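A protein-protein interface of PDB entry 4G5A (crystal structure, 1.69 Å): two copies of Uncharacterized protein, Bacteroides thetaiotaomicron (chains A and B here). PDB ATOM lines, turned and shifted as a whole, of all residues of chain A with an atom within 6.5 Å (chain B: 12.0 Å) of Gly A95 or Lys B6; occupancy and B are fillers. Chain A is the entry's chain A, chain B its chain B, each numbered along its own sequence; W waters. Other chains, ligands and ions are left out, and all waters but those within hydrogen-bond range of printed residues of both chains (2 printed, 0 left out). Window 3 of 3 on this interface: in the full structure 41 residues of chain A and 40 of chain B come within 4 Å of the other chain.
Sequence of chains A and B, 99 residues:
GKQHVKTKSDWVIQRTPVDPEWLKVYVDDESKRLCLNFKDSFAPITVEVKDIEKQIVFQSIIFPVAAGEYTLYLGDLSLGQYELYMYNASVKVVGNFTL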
ATOM      1  N   VAL A  25      -6.954  13.828  15.003  1.00  0.00           N
ATOM      2  CA  VAL A  25      -7.550  12.526  14.700  1.00  0.00           C
ATOM      3  C   VAL A  25      -7.382  12.222  13.201  1.00  0.00           C
ATOM      4  O   VAL A  25      -7.598  13.096  12.319  1.00  0.00           O
ATOM      5  CB  VAL A  25      -9.054  12.479  15.071  1.00  0.00           C
ATOM      6  CG1 VAL A  25      -9.671  11.078  14.741  1.00  0.00           C
ATOM      7  CG2 VAL A  25      -9.276  12.860  16.587  1.00  0.00           C
ATOM      8  N   TYR A  82     -19.659   7.649   9.162  1.00  0.00           N
ATOM      9  CA  TYR A  82     -19.708   7.542  10.616  1.00  0.00           C
ATOM     10  C   TYR A  82     -19.547   8.877  11.334  1.00  0.00           C
ATOM     11  O   TYR A  82     -18.878   9.781  10.820  1.00  0.00           O
ATOM     12  CB  TYR A  82     -18.620   6.589  11.117  1.00  0.00           C
ATOM     13  CG  TYR A  82     -18.858   5.177  10.663  1.00  0.00           C
ATOM     14  CD1 TYR A  82     -19.794   4.383  11.304  1.00  0.00           C
ATOM     15  CD2 TYR A  82     -18.207   4.650   9.544  1.00  0.00           C
ATOM     16  CE1 TYR A  82     -20.071   3.104  10.870  1.00  0.00           C
ATOM     17  CE2 TYR A  82     -18.471   3.354   9.121  1.00  0.00           C
ATOM     18  CZ  TYR A  82     -19.414   2.589   9.786  1.00  0.00           C
ATOM     19  OH  TYR A  82     -19.692   1.311   9.383  1.00  0.00           O
ATOM     20  N   GLU A  83     -20.174   8.984  12.503  1.00  0.00           N
ATOM     21  CA  GLU A  83     -19.972  10.119  13.405  1.00  0.00           C
ATOM     22  C   GLU A  83     -19.086   9.699  14.563  1.00  0.00           C
ATOM     23  O   GLU A  83     -19.347   8.669  15.203  1.00  0.00           O
ATOM     24  CB  GLU A  83     -21.280  10.642  14.003  1.00  0.00           C
ATOM     25  CG  GLU A  83     -21.039  11.883  14.906  1.00  0.00           C
ATOM     26  CD  GLU A  83     -22.172  12.187  15.899  1.00  0.00           C
ATOM     27  OE1 GLU A  83     -22.381  11.421  16.880  1.00  0.00           O
ATOM     28  OE2 GLU A  83     -22.828  13.223  15.686  1.00  0.00           O
ATOM     29  N   LEU A  84     -18.064  10.516  14.857  1.00  0.00           N
ATOM     30  CA  LEU A  84     -17.187  10.340  15.991  1.00  0.00           C
ATOM     31  C   LEU A  84     -17.596  11.304  17.114  1.00  0.00           C
ATOM     32  O   LEU A  84     -17.839  12.489  16.873  1.00  0.00           O
ATOM     33  CB  LEU A  84     -15.732  10.638  15.581  1.00  0.00           C
ATOM     34  CG  LEU A  84     -14.659  10.518  16.644  1.00  0.00           C
ATOM     35  CD1 LEU A  84     -14.560   9.087  17.138  1.00  0.00           C
ATOM     36  CD2 LEU A  84     -13.303  11.021  16.056  1.00  0.00           C
ATOM     37  N   TYR A  85     -17.737  10.781  18.320  1.00  0.00           N
ATOM     38  CA  TYR A  85     -18.071  11.585  19.509  1.00  0.00           C
ATOM     39  C   TYR A  85     -17.147  11.122  20.628  1.00  0.00           C
ATOM     40  O   TYR A  85     -17.077   9.933  20.951  1.00  0.00           O
ATOM     41  CB  TYR A  85     -19.550  11.392  19.894  1.00  0.00           C
ATOM     42  CG  TYR A  85     -20.001  12.114  21.141  1.00  0.00           C
ATOM     43  CD1 TYR A  85     -19.649  13.446  21.375  1.00  0.00           C
ATOM     44  CD2 TYR A  85     -20.840  11.474  22.064  1.00  0.00           C
ATOM     45  CE1 TYR A  85     -20.069  14.100  22.534  1.00  0.00           C
ATOM     46  CE2 TYR A  85     -21.290  12.132  23.201  1.00  0.00           C
ATOM     47  CZ  TYR A  85     -20.895  13.437  23.434  1.00  0.00           C
ATOM     48  OH  TYR A  85     -21.332  14.082  24.575  1.00  0.00           O
ATOM     49  N   VAL A  93     -15.934  16.323  21.849  1.00  0.00           N
ATOM     50  CA  VAL A  93     -15.305  16.438  20.544  1.00  0.00           C
ATOM     51  C   VAL A  93     -16.194  15.687  19.535  1.00  0.00           C
ATOM     52  O   VAL A  93     -16.653  14.571  19.810  1.00  0.00           O
ATOM     53  CB  VAL A  93     -13.886  15.849  20.514  1.00  0.00           C
ATOM     54  CG1 VAL A  93     -13.198  16.096  19.146  1.00  0.00           C
ATOM     55  CG2 VAL A  93     -13.014  16.408  21.624  1.00  0.00           C
ATOM     56  N   VAL A  94     -16.475  16.337  18.421  1.00  0.00           N
ATOM     57  CA  VAL A  94     -17.257  15.726  17.349  1.00  0.00           C
ATOM     58  C   VAL A  94     -16.556  15.847  15.989  1.00  0.00           C
ATOM     59  O   VAL A  94     -15.862  16.823  15.689  1.00  0.00           O
ATOM     60  CB  VAL A  94     -18.683  16.310  17.279  1.00  0.00           C
ATOM     61  CG1 VAL A  94     -19.520  15.563  16.226  1.00  0.00           C
ATOM     62  CG2 VAL A  94     -19.350  16.226  18.631  1.00  0.00           C
ATOM     63  N   GLY A  95     -16.719  14.810  15.177  1.00  0.00           N
ATOM     64  CA  GLY A  95     -16.219  14.782  13.825  1.00  0.00           C
ATOM     65  C   GLY A  95     -16.938  13.713  13.027  1.00  0.00           C
ATOM     66  O   GLY A  95     -17.758  12.989  13.548  1.00  0.00           O
ATOM     67  N   ASN A  96     -16.610  13.632  11.738  1.00  0.00           N
ATOM     68  CA  ASN A  96     -17.241  12.684  10.840  1.00  0.00           C
ATOM     69  C   ASN A  96     -16.167  12.074   9.950  1.00  0.00           C
ATOM     70  O   ASN A  96     -15.134  12.713   9.665  1.00  0.00           O
ATOM     71  CB  ASN A  96     -18.324  13.379   9.996  1.00  0.00           C
ATOM     72  CG  ASN A  96     -19.509  13.844  10.832  1.00  0.00           C
ATOM     73  OD1 ASN A  96     -20.390  13.056  11.174  1.00  0.00           O
ATOM     74  ND2 ASN A  96     -19.520  15.126  11.178  1.00  0.00           N
ATOM     75  N   PHE A  97     -16.366  10.816   9.559  1.00  0.00           N
ATOM     76  CA  PHE A  97     -15.426  10.171   8.661  1.00  0.00           C
ATOM     77  C   PHE A  97     -16.094   9.062   7.892  1.00  0.00           C
ATOM     78  O   PHE A  97     -17.213   8.655   8.202  1.00  0.00           O
ATOM     79  CB  PHE A  97     -14.225   9.614   9.418  1.00  0.00           C
ATOM     80  CG  PHE A  97     -14.551   8.528  10.407  1.00  0.00           C
ATOM     81  CD1 PHE A  97     -14.902   8.842  11.710  1.00  0.00           C
ATOM     82  CD2 PHE A  97     -14.475   7.191  10.046  1.00  0.00           C
ATOM     83  CE1 PHE A  97     -15.182   7.846  12.627  1.00  0.00           C
ATOM     84  CE2 PHE A  97     -14.755   6.184  10.956  1.00  0.00           C
ATOM     85  CZ  PHE A  97     -15.129   6.516  12.260  1.00  0.00           C
ATOM     86  N   LYS B   2      -4.279   7.203   5.095  1.00  0.00           N
ATOM     87  CA  LYS B   2      -4.459   7.970   6.344  1.00  0.00           C
ATOM     88  C   LYS B   2      -4.884   9.425   6.105  1.00  0.00           C
ATOM     89  O   LYS B   2      -4.172  10.187   5.464  1.00  0.00           O
ATOM     90  CB  LYS B   2      -3.171   7.935   7.160  1.00  0.00           C
ATOM     91  CG  LYS B   2      -3.293   8.516   8.564  1.00  0.00           C
ATOM     92  CD  LYS B   2      -2.162   8.031   9.453  1.00  0.00           C
ATOM     93  CE  LYS B   2      -2.232   8.614  10.855  1.00  0.00           C
ATOM     94  NZ  LYS B   2      -1.157   8.074  11.747  1.00  0.00           N
ATOM     95  N   GLN B   3      -6.043   9.810   6.641  1.00  0.00           N
ATOM     96  CA  GLN B   3      -6.631  11.113   6.400  1.00  0.00           C
ATOM     97  C   GLN B   3      -7.016  11.789   7.713  1.00  0.00           C
ATOM     98  O   GLN B   3      -7.535  11.125   8.609  1.00  0.00           O
ATOM     99  CB  GLN B   3      -7.868  10.940   5.540  1.00  0.00           C
ATOM    100  CG  GLN B   3      -8.554  12.222   5.113  1.00  0.00           C
ATOM    101  CD  GLN B   3      -9.469  12.015   3.934  1.00  0.00           C
ATOM    102  OE1 GLN B   3      -9.696  10.890   3.501  1.00  0.00           O
ATOM    103  NE2 GLN B   3      -9.979  13.107   3.390  1.00  0.00           N
ATOM    104  N   HIS B   4      -6.724  13.084   7.823  1.00  0.00           N
ATOM    105  CA  HIS B   4      -7.150  13.899   8.972  1.00  0.00           C
ATOM    106  C   HIS B   4      -8.660  13.996   9.042  1.00  0.00           C
ATOM    107  O   HIS B   4      -9.340  14.178   8.039  1.00  0.00           O
ATOM    108  CB  HIS B   4      -6.526  15.305   8.898  1.00  0.00           C
ATOM    109  CG  HIS B   4      -6.846  16.191  10.072  1.00  0.00           C
ATOM    110  ND1 HIS B   4      -7.574  17.358   9.949  1.00  0.00           N
ATOM    111  CD2 HIS B   4      -6.514  16.093  11.385  1.00  0.00           C
ATOM    112  CE1 HIS B   4      -7.682  17.937  11.134  1.00  0.00           C
ATOM    113  NE2 HIS B   4      -7.040  17.195  12.021  1.00  0.00           N
ATOM    114  N   VAL B   5      -9.197  13.800  10.252  1.00  0.00           N
ATOM    115  CA  VAL B   5     -10.615  13.932  10.494  1.00  0.00           C
ATOM    116  C   VAL B   5     -10.776  15.270  11.192  1.00  0.00           C
ATOM    117  O   VAL B   5     -10.207  15.444  12.255  1.00  0.00           O
ATOM    118  CB  VAL B   5     -11.153  12.803  11.428  1.00  0.00           C
ATOM    119  CG1 VAL B   5     -12.618  13.097  11.846  1.00  0.00           C
ATOM    120  CG2 VAL B   5     -11.001  11.435  10.754  1.00  0.00           C
ATOM    121  N   LYS B   6     -11.491  16.214  10.577  1.00  0.00           N
ATOM    122  CA  LYS B   6     -11.656  17.530  11.182  1.00  0.00           C
ATOM    123  C   LYS B   6     -12.556  17.385  12.403  1.00  0.00           C
ATOM    124  O   LYS B   6     -13.640  16.825  12.321  1.00  0.00           O
ATOM    125  CB  LYS B   6     -12.223  18.548  10.188  1.00  0.00           C
ATOM    126  CG  LYS B   6     -11.195  19.058   9.178  1.00  0.00           C
ATOM    127  N   THR B   7     -12.064  17.861  13.542  1.00  0.00           N
ATOM    128  CA  THR B   7     -12.808  17.756  14.781  1.00  0.00           C
ATOM    129  C   THR B   7     -13.082  19.144  15.349  1.00  0.00           C
ATOM    130  O   THR B   7     -12.287  20.077  15.152  1.00  0.00           O
ATOM    131  CB  THR B   7     -12.080  16.873  15.824  1.00  0.00           C
ATOM    132  OG1 THR B   7     -10.750  17.359  16.087  1.00  0.00           O
ATOM    133  CG2 THR B   7     -12.036  15.430  15.367  1.00  0.00           C
ATOM    134  N   LYS B   8     -14.229  19.272  16.014  1.00  0.00           N
ATOM    135  CA  LYS B   8     -14.583  20.479  16.746  1.00  0.00           C
ATOM    136  C   LYS B   8     -14.633  20.107  18.229  1.00  0.00           C
ATOM    137  O   LYS B   8     -15.337  19.160  18.614  1.00  0.00           O
ATOM    138  CB  LYS B   8     -15.946  20.980  16.279  1.00  0.00           C
ATOM    139  CG  LYS B   8     -16.361  22.350  16.813  1.00  0.00           C
ATOM    140  CD  LYS B   8     -17.719  22.779  16.197  1.00  0.00           C
ATOM    141  CE  LYS B   8     -18.127  24.217  16.564  1.00  0.00           C
ATOM    142  NZ  LYS B   8     -17.575  25.278  15.654  1.00  0.00           N
ATOM    143  N   SER B   9     -13.907  20.872  19.034  1.00  0.00           N
ATOM    144  CA  SER B   9     -13.840  20.662  20.489  1.00  0.00           C
ATOM    145  C   SER B   9     -14.670  21.722  21.201  1.00  0.00           C
ATOM    146  O   SER B   9     -14.563  22.913  20.890  1.00  0.00           O
ATOM    147  CB  SER B   9     -12.389  20.711  20.965  1.00  0.00           C
ATOM    148  OG  SER B   9     -11.633  19.630  20.403  1.00  0.00           O
ATOM    149  N   ASP B  10     -15.463  21.278  22.167  1.00  0.00           N
ATOM    150  CA  ASP B  10     -16.193  22.152  23.064  1.00  0.00           C
ATOM    151  C   ASP B  10     -15.673  21.958  24.484  1.00  0.00           C
ATOM    152  O   ASP B  10     -15.974  20.946  25.135  1.00  0.00           O
ATOM    153  CB  ASP B  10     -17.666  21.809  23.033  1.00  0.00           C
ATOM    154  CG  ASP B  10     -18.482  22.645  23.997  1.00  0.00           C
ATOM    155  OD1 ASP B  10     -17.943  23.656  24.517  1.00  0.00           O
ATOM    156  OD2 ASP B  10     -19.640  22.258  24.266  1.00  0.00           O
HETATM  157  O   HOH W   1      -8.636  16.091  14.388  1.00  0.00           O
HETATM  158  O   HOH W   2     -15.230  15.911  10.495  1.00  0.00           O
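Val A25 touches three residues of chain B.
No residue of chain B comes within 4 Å of Leu A84.
Tyr A85 touches none of the printed residues of chain B.
Of the printed residues of chain B, Asn A96 touches Val B5.
Phe A97 touches one residue of chain B.
Of the printed residues of chain A, His B4 touches Val A25.
Printed residues of chain A within 4 Å of Val B5: Val A25, Asn A96 and Phe A97.
Of the printed residues of chain A, Thr B7 touches Val A25 (3.96 Å), Val A93 (3.6 Å) and Val A94 (3.3 Å).
Of the printed residues of chain A, Lys B8 touches Val A93 and Val A94.
Asp B10 touches none of the printed residues of chain A.
The nearest printed residue of chain B that does not touch Gly A95 is Val B5 (4.4 Å).
The nearest printed residue of chain A that does not touch His B4 is Asn A96 (6.2 Å).
Printed residues of chain B that touch a printed residue of chain A: His B4, Val B5, Lys B6, Thr B7, Lys B8 and Ser B9.
Hydrophobic or aromatic side chains of chain B that line the printed part of chain A: His B4 and Val B5.
Hydrophobic or aromatic side chains of chain A that line the printed part of chain B: Val A25, Val A93 and Phe A97.
No position is printed for both chains.
Of the 11 pairs that touch across the chains among the printed residues, none has its exchanged pair printed and touching as well.
The backbone NH (N) of Tyr A82 lies within hydrogen-bond range of the backbone carbonyl oxygen (O) of Phe A97, at 2.8 Å.
The backbone NH (N) of Leu A84 lies within hydrogen-bond range of the backbone carbonyl oxygen (O) of Gly A95, 2.8 Å away.
Water W2 lies within hydrogen-bond range of the backbone carbonyl oxygen (O) of Lys B6 (2.6 Å) and the backbone NH (N) of Asn A96 (2.9 Å).
Water W1 lies within hydrogen-bond range of the backbone carbonyl oxygen of Val B5, the backbone NH of Val A25, the side-chain hydroxyl of Thr B7 and a ring nitrogen (NE2) of His B4.
O of Val A25 touches CD2 of His B4, 3.3 Å away.
Thr B7 touches Val A25 (CG2 to CG2, 3.96 Å).
Val A93 touches Thr B7 (CG1 to CB, 3.6 Å).
CA of Val A93 touches O of Lys B8, 3.3 Å away.
CG2 of Val A93 touches OG of Ser B9, at 3.7 Å.
Val A94 touches Thr B7.
Gly A95 touches Lys B6 (CA to O, 3.6 Å).
Asn A96 touches Val B5 (O to CG1, 3.4 Å).
Phe A97 touches Val B5 (CB to CG2, 3.9 Å).
The backbone NH (N) of Val B5 is in hydrogen-bond range of the backbone carbonyl oxygen (O) of Val A25, at 2.7 Å.
The backbone carbonyl oxygen of Val A94 is in hydrogen-bond range of the backbone NH of Lys B8.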
